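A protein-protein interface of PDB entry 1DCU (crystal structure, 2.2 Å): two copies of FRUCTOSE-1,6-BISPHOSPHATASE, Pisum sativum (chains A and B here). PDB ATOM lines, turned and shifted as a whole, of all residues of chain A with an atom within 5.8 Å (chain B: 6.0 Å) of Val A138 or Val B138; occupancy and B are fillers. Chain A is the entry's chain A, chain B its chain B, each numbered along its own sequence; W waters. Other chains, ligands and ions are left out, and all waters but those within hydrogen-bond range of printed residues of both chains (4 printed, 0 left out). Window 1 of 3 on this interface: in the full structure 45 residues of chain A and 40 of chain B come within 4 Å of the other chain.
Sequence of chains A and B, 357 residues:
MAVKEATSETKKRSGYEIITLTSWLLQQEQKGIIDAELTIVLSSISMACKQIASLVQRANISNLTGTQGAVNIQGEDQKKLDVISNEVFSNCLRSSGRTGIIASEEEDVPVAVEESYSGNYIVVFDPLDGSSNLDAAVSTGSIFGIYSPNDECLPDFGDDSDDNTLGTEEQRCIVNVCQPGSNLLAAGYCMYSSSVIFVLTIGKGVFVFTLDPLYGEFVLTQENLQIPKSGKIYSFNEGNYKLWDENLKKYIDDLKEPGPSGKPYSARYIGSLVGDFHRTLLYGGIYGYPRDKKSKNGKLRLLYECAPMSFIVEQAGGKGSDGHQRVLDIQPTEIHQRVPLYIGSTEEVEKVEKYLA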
ATOM      1  N   LEU A 134     -25.284 -23.618  11.286  1.00  0.00           N
ATOM      2  CA  LEU A 134     -25.182 -23.008   9.967  1.00  0.00           C
ATOM      3  C   LEU A 134     -23.745 -23.216   9.499  1.00  0.00           C
ATOM      4  O   LEU A 134     -23.580 -23.732   8.440  1.00  0.00           O
ATOM      5  CB  LEU A 134     -25.403 -21.480  10.059  1.00  0.00           C
ATOM      6  CG  LEU A 134     -25.146 -20.751   8.750  1.00  0.00           C
ATOM      7  CD1 LEU A 134     -26.186 -21.105   7.681  1.00  0.00           C
ATOM      8  CD2 LEU A 134     -25.228 -19.260   9.060  1.00  0.00           C
ATOM      9  N   ASP A 135     -22.783 -22.919  10.372  1.00  0.00           N
ATOM     10  CA  ASP A 135     -21.405 -22.913   9.999  1.00  0.00           C
ATOM     11  C   ASP A 135     -20.766 -24.320   9.916  1.00  0.00           C
ATOM     12  O   ASP A 135     -19.625 -24.431   9.463  1.00  0.00           O
ATOM     13  CB  ASP A 135     -20.559 -22.125  10.990  1.00  0.00           C
ATOM     14  CG  ASP A 135     -20.906 -20.636  10.961  1.00  0.00           C
ATOM     15  OD1 ASP A 135     -20.530 -20.027  11.997  1.00  0.00           O
ATOM     16  OD2 ASP A 135     -21.474 -20.169   9.982  1.00  0.00           O
ATOM     17  N   ALA A 136     -21.501 -25.316  10.369  1.00  0.00           N
ATOM     18  CA  ALA A 136     -20.999 -26.677  10.332  1.00  0.00           C
ATOM     19  C   ALA A 136     -21.810 -27.527   9.365  1.00  0.00           C
ATOM     20  O   ALA A 136     -21.676 -28.745   9.302  1.00  0.00           O
ATOM     21  CB  ALA A 136     -21.057 -27.279  11.730  1.00  0.00           C
ATOM     22  N   ALA A 137     -22.547 -26.834   8.531  1.00  0.00           N
ATOM     23  CA  ALA A 137     -23.400 -27.469   7.549  1.00  0.00           C
ATOM     24  C   ALA A 137     -22.594 -28.429   6.686  1.00  0.00           C
ATOM     25  O   ALA A 137     -23.274 -29.404   6.228  1.00  0.00           O
ATOM     26  CB  ALA A 137     -24.136 -26.457   6.669  1.00  0.00           C
ATOM     27  N   VAL A 138     -21.402 -27.987   6.209  1.00  0.00           N
ATOM     28  CA  VAL A 138     -20.682 -28.901   5.349  1.00  0.00           C
ATOM     29  C   VAL A 138     -19.345 -29.358   5.907  1.00  0.00           C
ATOM     30  O   VAL A 138     -18.720 -30.331   5.407  1.00  0.00           O
ATOM     31  CB  VAL A 138     -20.414 -28.383   3.951  1.00  0.00           C
ATOM     32  CG1 VAL A 138     -21.779 -28.093   3.328  1.00  0.00           C
ATOM     33  CG2 VAL A 138     -19.429 -27.226   4.153  1.00  0.00           C
ATOM     34  N   SER A 139     -18.760 -28.646   6.839  1.00  0.00           N
ATOM     35  CA  SER A 139     -17.486 -29.022   7.387  1.00  0.00           C
ATOM     36  C   SER A 139     -17.256 -28.452   8.764  1.00  0.00           C
ATOM     37  O   SER A 139     -17.764 -27.447   9.204  1.00  0.00           O
ATOM     38  CB  SER A 139     -16.238 -28.673   6.574  1.00  0.00           C
ATOM     39  OG  SER A 139     -16.117 -27.282   6.704  1.00  0.00           O
ATOM     40  N   THR A 140     -16.443 -29.192   9.510  1.00  0.00           N
ATOM     41  CA  THR A 140     -16.118 -28.709  10.857  1.00  0.00           C
ATOM     42  C   THR A 140     -14.784 -29.396  11.160  1.00  0.00           C
ATOM     43  O   THR A 140     -14.220 -29.983  10.217  1.00  0.00           O
ATOM     44  CB  THR A 140     -17.195 -29.103  11.871  1.00  0.00           C
ATOM     45  OG1 THR A 140     -16.825 -28.604  13.179  1.00  0.00           O
ATOM     46  CG2 THR A 140     -17.361 -30.609  11.973  1.00  0.00           C
ATOM     47  N   MET A 191      -9.887 -32.163   9.912  1.00  0.00           N
ATOM     48  CA  MET A 191     -11.106 -31.632   9.303  1.00  0.00           C
ATOM     49  C   MET A 191     -12.103 -32.691   8.927  1.00  0.00           C
ATOM     50  O   MET A 191     -11.759 -33.744   8.400  1.00  0.00           O
ATOM     51  CB  MET A 191     -10.639 -30.906   8.015  1.00  0.00           C
ATOM     52  CG  MET A 191     -11.803 -30.478   7.174  1.00  0.00           C
ATOM     53  SD  MET A 191     -11.434 -29.552   5.702  1.00  0.00           S
ATOM     54  CE  MET A 191     -10.677 -30.865   4.727  1.00  0.00           C
ATOM     55  N   TYR A 192     -13.348 -32.488   9.271  1.00  0.00           N
ATOM     56  CA  TYR A 192     -14.400 -33.452   8.979  1.00  0.00           C
ATOM     57  C   TYR A 192     -15.236 -32.841   7.869  1.00  0.00           C
ATOM     58  O   TYR A 192     -15.953 -31.861   8.129  1.00  0.00           O
ATOM     59  CB  TYR A 192     -15.258 -33.769  10.186  1.00  0.00           C
ATOM     60  CG  TYR A 192     -14.438 -33.949  11.442  1.00  0.00           C
ATOM     61  CD1 TYR A 192     -13.568 -35.010  11.528  1.00  0.00           C
ATOM     62  CD2 TYR A 192     -14.480 -33.079  12.554  1.00  0.00           C
ATOM     63  CE1 TYR A 192     -12.746 -35.212  12.667  1.00  0.00           C
ATOM     64  CE2 TYR A 192     -13.708 -33.249  13.697  1.00  0.00           C
ATOM     65  CZ  TYR A 192     -12.837 -34.328  13.726  1.00  0.00           C
ATOM     66  OH  TYR A 192     -12.087 -34.592  14.823  1.00  0.00           O
ATOM     67  N   SER A 193     -15.017 -33.252   6.636  1.00  0.00           N
ATOM     68  CA  SER A 193     -15.698 -32.727   5.456  1.00  0.00           C
ATOM     69  C   SER A 193     -15.865 -33.841   4.440  1.00  0.00           C
ATOM     70  O   SER A 193     -16.064 -34.986   4.930  1.00  0.00           O
ATOM     71  CB  SER A 193     -14.946 -31.550   4.825  1.00  0.00           C
ATOM     72  OG  SER A 193     -13.748 -32.115   4.328  1.00  0.00           O
ATOM     73  N   SER A 194     -15.886 -33.620   3.131  1.00  0.00           N
ATOM     74  CA  SER A 194     -16.068 -34.762   2.212  1.00  0.00           C
ATOM     75  C   SER A 194     -14.980 -35.808   2.357  1.00  0.00           C
ATOM     76  O   SER A 194     -15.275 -36.920   1.983  1.00  0.00           O
ATOM     77  CB  SER A 194     -16.043 -34.400   0.733  1.00  0.00           C
ATOM     78  OG  SER A 194     -15.147 -33.396   0.525  1.00  0.00           O
ATOM     79  N   SER A 195     -13.807 -35.453   2.891  1.00  0.00           N
ATOM     80  CA  SER A 195     -12.874 -36.348   3.412  1.00  0.00           C
ATOM     81  C   SER A 195     -12.505 -35.903   4.838  1.00  0.00           C
ATOM     82  O   SER A 195     -12.765 -34.764   5.246  1.00  0.00           O
ATOM     83  CB  SER A 195     -11.629 -36.466   2.503  1.00  0.00           C
ATOM     84  OG  SER A 195     -11.074 -35.150   2.544  1.00  0.00           O
ATOM     85  N   ILE A 270     -16.483 -20.527   3.918  1.00  0.00           N
ATOM     86  CA  ILE A 270     -17.383 -21.620   4.367  1.00  0.00           C
ATOM     87  C   ILE A 270     -18.051 -21.182   5.646  1.00  0.00           C
ATOM     88  O   ILE A 270     -19.223 -21.388   5.896  1.00  0.00           O
ATOM     89  CB  ILE A 270     -16.663 -22.957   4.606  1.00  0.00           C
ATOM     90  CG1 ILE A 270     -15.970 -23.322   3.324  1.00  0.00           C
ATOM     91  CG2 ILE A 270     -17.669 -24.009   5.166  1.00  0.00           C
ATOM     92  CD1 ILE A 270     -14.701 -24.225   3.549  1.00  0.00           C
ATOM     93  N   GLY A 275     -12.292 -25.622   7.828  1.00  0.00           N
ATOM     94  CA  GLY A 275     -12.579 -25.741   6.413  1.00  0.00           C
ATOM     95  C   GLY A 275     -11.922 -24.605   5.629  1.00  0.00           C
ATOM     96  O   GLY A 275     -11.220 -24.831   4.630  1.00  0.00           O
ATOM     97  N   ASP A 276     -12.219 -23.381   6.045  1.00  0.00           N
ATOM     98  CA  ASP A 276     -11.630 -22.192   5.393  1.00  0.00           C
ATOM     99  C   ASP A 276     -10.102 -22.133   5.468  1.00  0.00           C
ATOM    100  O   ASP A 276      -9.479 -21.814   4.455  1.00  0.00           O
ATOM    101  CB  ASP A 276     -12.265 -20.953   5.976  1.00  0.00           C
ATOM    102  CG  ASP A 276     -13.687 -20.640   5.518  1.00  0.00           C
ATOM    103  OD1 ASP A 276     -13.903 -20.710   4.309  1.00  0.00           O
ATOM    104  OD2 ASP A 276     -14.493 -20.301   6.424  1.00  0.00           O
ATOM    105  N   LEU B 134     -10.720 -26.393  -6.075  1.00  0.00           N
ATOM    106  CA  LEU B 134     -10.862 -25.335  -5.169  1.00  0.00           C
ATOM    107  C   LEU B 134     -12.292 -25.397  -4.611  1.00  0.00           C
ATOM    108  O   LEU B 134     -12.485 -25.213  -3.443  1.00  0.00           O
ATOM    109  CB  LEU B 134     -10.560 -23.959  -5.811  1.00  0.00           C
ATOM    110  CG  LEU B 134     -10.880 -22.816  -4.825  1.00  0.00           C
ATOM    111  CD1 LEU B 134      -9.719 -22.799  -3.796  1.00  0.00           C
ATOM    112  CD2 LEU B 134     -11.086 -21.502  -5.507  1.00  0.00           C
ATOM    113  N   ASP B 135     -13.260 -25.460  -5.456  1.00  0.00           N
ATOM    114  CA  ASP B 135     -14.656 -25.562  -5.111  1.00  0.00           C
ATOM    115  C   ASP B 135     -15.129 -26.881  -4.508  1.00  0.00           C
ATOM    116  O   ASP B 135     -16.210 -26.838  -3.924  1.00  0.00           O
ATOM    117  CB  ASP B 135     -15.477 -25.323  -6.387  1.00  0.00           C
ATOM    118  CG  ASP B 135     -15.242 -23.909  -6.885  1.00  0.00           C
ATOM    119  OD1 ASP B 135     -14.698 -23.047  -6.174  1.00  0.00           O
ATOM    120  OD2 ASP B 135     -15.620 -23.679  -8.038  1.00  0.00           O
ATOM    121  N   ALA B 136     -14.408 -27.964  -4.588  1.00  0.00           N
ATOM    122  CA  ALA B 136     -14.613 -29.257  -4.040  1.00  0.00           C
ATOM    123  C   ALA B 136     -13.731 -29.505  -2.807  1.00  0.00           C
ATOM    124  O   ALA B 136     -13.687 -30.646  -2.297  1.00  0.00           O
ATOM    125  CB  ALA B 136     -14.197 -30.440  -5.026  1.00  0.00           C
ATOM    126  N   ALA B 137     -13.178 -28.465  -2.229  1.00  0.00           N
ATOM    127  CA  ALA B 137     -12.274 -28.703  -1.094  1.00  0.00           C
ATOM    128  C   ALA B 137     -12.944 -29.386   0.083  1.00  0.00           C
ATOM    129  O   ALA B 137     -12.213 -30.076   0.802  1.00  0.00           O
ATOM    130  CB  ALA B 137     -11.610 -27.406  -0.606  1.00  0.00           C
ATOM    131  N   VAL B 138     -14.189 -28.967   0.374  1.00  0.00           N
ATOM    132  CA  VAL B 138     -14.830 -29.500   1.538  1.00  0.00           C
ATOM    133  C   VAL B 138     -16.153 -30.196   1.156  1.00  0.00           C
ATOM    134  O   VAL B 138     -16.574 -31.008   1.933  1.00  0.00           O
ATOM    135  CB  VAL B 138     -15.154 -28.430   2.615  1.00  0.00           C
ATOM    136  CG1 VAL B 138     -13.861 -27.912   3.258  1.00  0.00           C
ATOM    137  CG2 VAL B 138     -16.150 -27.434   2.144  1.00  0.00           C
ATOM    138  N   SER B 139     -16.721 -29.909  -0.021  1.00  0.00           N
ATOM    139  CA  SER B 139     -17.928 -30.559  -0.376  1.00  0.00           C
ATOM    140  C   SER B 139     -18.173 -30.587  -1.826  1.00  0.00           C
ATOM    141  O   SER B 139     -17.653 -29.821  -2.642  1.00  0.00           O
ATOM    142  CB  SER B 139     -19.160 -29.845   0.303  1.00  0.00           C
ATOM    143  OG  SER B 139     -19.183 -28.569  -0.249  1.00  0.00           O
ATOM    144  N   THR B 140     -19.039 -31.558  -2.167  1.00  0.00           N
ATOM    145  CA  THR B 140     -19.363 -31.699  -3.615  1.00  0.00           C
ATOM    146  C   THR B 140     -20.657 -32.496  -3.594  1.00  0.00           C
ATOM    147  O   THR B 140     -21.195 -32.741  -2.474  1.00  0.00           O
ATOM    148  CB  THR B 140     -18.197 -32.284  -4.436  1.00  0.00           C
ATOM    149  OG1 THR B 140     -18.643 -32.214  -5.843  1.00  0.00           O
ATOM    150  CG2 THR B 140     -17.821 -33.751  -4.132  1.00  0.00           C
ATOM    151  N   MET B 191     -25.296 -34.945  -1.399  1.00  0.00           N
ATOM    152  CA  MET B 191     -24.173 -34.068  -1.053  1.00  0.00           C
ATOM    153  C   MET B 191     -23.071 -34.972  -0.399  1.00  0.00           C
ATOM    154  O   MET B 191     -23.418 -35.758   0.509  1.00  0.00           O
ATOM    155  CB  MET B 191     -24.655 -33.117   0.038  1.00  0.00           C
ATOM    156  CG  MET B 191     -23.432 -32.294   0.573  1.00  0.00           C
ATOM    157  SD  MET B 191     -24.067 -30.961   1.594  1.00  0.00           S
ATOM    158  CE  MET B 191     -24.361 -31.674   3.106  1.00  0.00           C
ATOM    159  N   TYR B 192     -21.838 -34.793  -0.797  1.00  0.00           N
ATOM    160  CA  TYR B 192     -20.736 -35.519  -0.142  1.00  0.00           C
ATOM    161  C   TYR B 192     -19.968 -34.455   0.662  1.00  0.00           C
ATOM    162  O   TYR B 192     -19.324 -33.575   0.123  1.00  0.00           O
ATOM    163  CB  TYR B 192     -19.778 -36.138  -1.206  1.00  0.00           C
ATOM    164  CG  TYR B 192     -20.589 -36.832  -2.287  1.00  0.00           C
ATOM    165  CD1 TYR B 192     -21.260 -37.969  -1.921  1.00  0.00           C
ATOM    166  CD2 TYR B 192     -20.657 -36.429  -3.597  1.00  0.00           C
ATOM    167  CE1 TYR B 192     -22.027 -38.695  -2.826  1.00  0.00           C
ATOM    168  CE2 TYR B 192     -21.454 -37.101  -4.552  1.00  0.00           C
ATOM    169  CZ  TYR B 192     -22.109 -38.255  -4.130  1.00  0.00           C
ATOM    170  OH  TYR B 192     -22.973 -38.926  -4.974  1.00  0.00           O
ATOM    171  N   SER B 193     -20.112 -34.518   2.001  1.00  0.00           N
ATOM    172  CA  SER B 193     -19.404 -33.530   2.810  1.00  0.00           C
ATOM    173  C   SER B 193     -19.240 -34.139   4.153  1.00  0.00           C
ATOM    174  O   SER B 193     -19.070 -35.378   4.240  1.00  0.00           O
ATOM    175  CB  SER B 193     -20.183 -32.181   2.892  1.00  0.00           C
ATOM    176  OG  SER B 193     -21.352 -32.340   3.711  1.00  0.00           O
ATOM    177  N   SER B 194     -19.205 -33.399   5.281  1.00  0.00           N
ATOM    178  CA  SER B 194     -18.992 -34.091   6.562  1.00  0.00           C
ATOM    179  C   SER B 194     -19.932 -35.214   6.906  1.00  0.00           C
ATOM    180  O   SER B 194     -19.764 -36.158   7.692  1.00  0.00           O
ATOM    181  CB  SER B 194     -18.855 -33.066   7.739  1.00  0.00           C
ATOM    182  OG  SER B 194     -20.113 -32.399   7.815  1.00  0.00           O
ATOM    183  N   SER B 195     -21.071 -35.233   6.187  1.00  0.00           N
ATOM    184  CA  SER B 195     -22.086 -36.282   6.235  1.00  0.00           C
ATOM    185  C   SER B 195     -22.471 -36.492   4.799  1.00  0.00           C
ATOM    186  O   SER B 195     -22.225 -35.652   3.907  1.00  0.00           O
ATOM    187  CB  SER B 195     -23.223 -35.815   7.184  1.00  0.00           C
ATOM    188  OG  SER B 195     -23.870 -34.742   6.589  1.00  0.00           O
ATOM    189  N   ILE B 270     -19.568 -21.352  -0.253  1.00  0.00           N
ATOM    190  CA  ILE B 270     -18.592 -22.439  -0.226  1.00  0.00           C
ATOM    191  C   ILE B 270     -17.888 -22.527  -1.580  1.00  0.00           C
ATOM    192  O   ILE B 270     -16.776 -23.004  -1.704  1.00  0.00           O
ATOM    193  CB  ILE B 270     -19.310 -23.777   0.138  1.00  0.00           C
ATOM    194  CG1 ILE B 270     -19.941 -23.692   1.520  1.00  0.00           C
ATOM    195  CG2 ILE B 270     -18.225 -24.908   0.059  1.00  0.00           C
ATOM    196  CD1 ILE B 270     -21.102 -24.658   1.820  1.00  0.00           C
ATOM    197  N   GLY B 275     -23.425 -28.003  -1.802  1.00  0.00           N
ATOM    198  CA  GLY B 275     -23.187 -27.574  -0.444  1.00  0.00           C
ATOM    199  C   GLY B 275     -23.948 -26.279  -0.090  1.00  0.00           C
ATOM    200  O   GLY B 275     -24.479 -26.128   1.017  1.00  0.00           O
ATOM    201  N   ASP B 276     -23.792 -25.246  -0.918  1.00  0.00           N
ATOM    202  CA  ASP B 276     -24.405 -23.951  -0.736  1.00  0.00           C
ATOM    203  C   ASP B 276     -25.953 -24.078  -0.916  1.00  0.00           C
ATOM    204  O   ASP B 276     -26.699 -23.510  -0.152  1.00  0.00           O
ATOM    205  CB  ASP B 276     -23.915 -22.920  -1.750  1.00  0.00           C
ATOM    206  CG  ASP B 276     -22.513 -22.298  -1.432  1.00  0.00           C
ATOM    207  OD1 ASP B 276     -22.184 -21.963  -0.289  1.00  0.00           O
ATOM    208  OD2 ASP B 276     -21.697 -22.241  -2.387  1.00  0.00           O
ATOM    209  N   HIS B 278     -27.657 -26.828  -0.350  1.00  0.00           N
ATOM    210  CA  HIS B 278     -28.093 -27.567   0.839  1.00  0.00           C
ATOM    211  C   HIS B 278     -28.206 -26.655   2.047  1.00  0.00           C
ATOM    212  O   HIS B 278     -29.168 -26.830   2.813  1.00  0.00           O
ATOM    213  CB  HIS B 278     -27.211 -28.735   1.185  1.00  0.00           C
ATOM    214  CG  HIS B 278     -27.664 -29.628   2.306  1.00  0.00           C
ATOM    215  ND1 HIS B 278     -28.718 -30.496   2.128  1.00  0.00           N
ATOM    216  CD2 HIS B 278     -27.196 -29.757   3.599  1.00  0.00           C
ATOM    217  CE1 HIS B 278     -28.866 -31.133   3.298  1.00  0.00           C
ATOM    218  NE2 HIS B 278     -28.000 -30.759   4.127  1.00  0.00           N
ATOM    219  N   ARG B 279     -27.232 -25.867   2.395  1.00  0.00           N
ATOM    220  CA  ARG B 279     -27.224 -24.980   3.543  1.00  0.00           C
ATOM    221  C   ARG B 279     -28.442 -24.001   3.454  1.00  0.00           C
ATOM    222  O   ARG B 279     -29.075 -23.732   4.487  1.00  0.00           O
ATOM    223  CB  ARG B 279     -25.951 -24.158   3.604  1.00  0.00           C
ATOM    224  CG  ARG B 279     -25.791 -23.253   4.859  1.00  0.00           C
ATOM    225  CD  ARG B 279     -24.755 -22.159   4.736  1.00  0.00           C
ATOM    226  NE  ARG B 279     -25.042 -21.384   3.576  1.00  0.00           N
ATOM    227  CZ  ARG B 279     -24.458 -21.357   2.404  1.00  0.00           C
ATOM    228  NH1 ARG B 279     -23.334 -22.030   2.157  1.00  0.00           N
ATOM    229  NH2 ARG B 279     -25.064 -20.684   1.435  1.00  0.00           N
HETATM  230  O   HOH W   1     -16.907 -36.622   7.801  1.00  0.00           O
HETATM  231  O   HOH W   2     -18.118 -37.745   2.131  1.00  0.00           O
HETATM  232  O   HOH W   3     -20.171 -30.964  10.060  1.00  0.00           O
HETATM  233  O   HOH W   4     -15.241 -32.864  -1.982  1.00  0.00           O
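The side-chain hydroxyl (OG) of Ser A193 sits at hydrogen-bond distance from the backbone carbonyl oxygen (O) of Ser A195.
OD1 of Asp A276 sits at hydrogen-bond distance from N of Ile A270 (2.6 Å).
The backbone carbonyl oxygen (O) of Thr B140 lies within hydrogen-bond range of the backbone NH (N) of Tyr B192 (2.7 Å).
The side-chain hydroxyl (OG) of Ser B193 sits close to the backbone carbonyl oxygen (O) of Ser B195.
OD1 of Asp B276 is in hydrogen-bond range of N of Ile B270 (2.7 Å).
The side-chain carboxylate (OD1) of Asp B276 is in salt-bridge range of the guanidinium group (NH1) of Arg B279 (2.7 Å).
Val A138 touches its own counterpart, Val B138.
Met A191 touches Val B138, but with the chains exchanged Val A138 does not touch Met B191 (4.1 Å).
Ser A194 touches Ser B139, but with the chains exchanged Ser A139 does not touch Ser B194 (4.1 Å).
Ser A194 touches its own counterpart, Ser B194.
Of the 16 pairs that touch across the chains among the printed residues, 13 have their exchanged pair printed and touching as well.
Of the 15 printed residues of chain A, 7 touch a printed residue of chain B.
Printed residues of chain A that touch a printed residue of chain B: Leu A134, Val A138, Met A191, Tyr A192, Ser A193, Ser A194 and Ile A270.
Hydrophobic or aromatic side chains of chain A that line the printed part of chain B: Leu A134, Val A138, Met A191 and Ile A270.
Printed residues of chain B that touch a printed residue of chain A: Val B138, Ser B139, Tyr B192, Ser B193, Ser B194, Ile B270 and Arg B279.
Hydrophobic or aromatic side chains of chain B within 4 Å of the printed part of chain A: Val B138 and Ile B270.
Among the printed residues, no Asp or Glu carboxylate lies within 4 Å of a Lys or Arg side-chain nitrogen of the other chain.
CD1 of Leu A134 touches CD of Arg B279, 3.4 Å away.
Val A138 touches Val B138.
Ile B270 touches Val A138 (CD1 to CG1, 3.8 Å).
Tyr A192 touches Ser B194 (O to CB, 3.2 Å).
Ser A193 touches Val B138 (CB to O, 3.4 Å).
O of Ser A193 touches CA of Ser B194 (3.5 Å).
N of Ser B139 touches OG of Ser A194 (3.9 Å).
N of Ser A194 touches CA of Ser B193, at 3.5 Å.
N of Ser A194 touches N of Ser B194 (3.96 Å).
Ile A270 touches Val B138.
O of Val A138 lies within hydrogen-bond range of N of Ser B194.
N of Ser A194 is in hydrogen-bond range of O of Val B138 (3.0 Å).
O of Ser B193 sits close to O of Ser A193, 3.1 Å away.
Val A138 touches just these residues of chain B: Val B138 (3.9 Å), Ser B193 (3.4 Å), Ser B194 (3.1 Å) and Ile B270 (3.8 Å).
Of the printed residues of chain A, Ile B270 touches Val A138 (3.8 Å).
Of the printed residues of chain A, Tyr B192 touches Ser A194 (3.4 Å).
Printed residues of chain B within 4 Å of Ser A193: Val B138 (3.4 Å), Ser B193 (3.1 Å) and Ser B194 (3.5 Å).
Of the printed residues of chain A, Arg B279 touches Leu A134.
Ala A137 touches none of the printed residues of chain B.
Ser B195 touches none of the printed residues of chain A.
The nearest printed residue of chain A that does not touch Ile B270 is Ile A270 (4.3 Å).
Water W4 bridges OG of Ser A194 (2.6 Å) and O of Ala B136 (2.7 Å).
Water W3 bridges the side-chain hydroxyl of Ser B194 (2.7 Å) and the backbone carbonyl oxygen of Ala A136 (2.8 Å).
Water W1 bridges O of Ser B194 (2.9 Å) and O of Ser A193 (3.4 Å).
Water W2 lies within hydrogen-bond range of O of Ser A194 (3.0 Å) and O of Ser B193 (3.3 Å).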
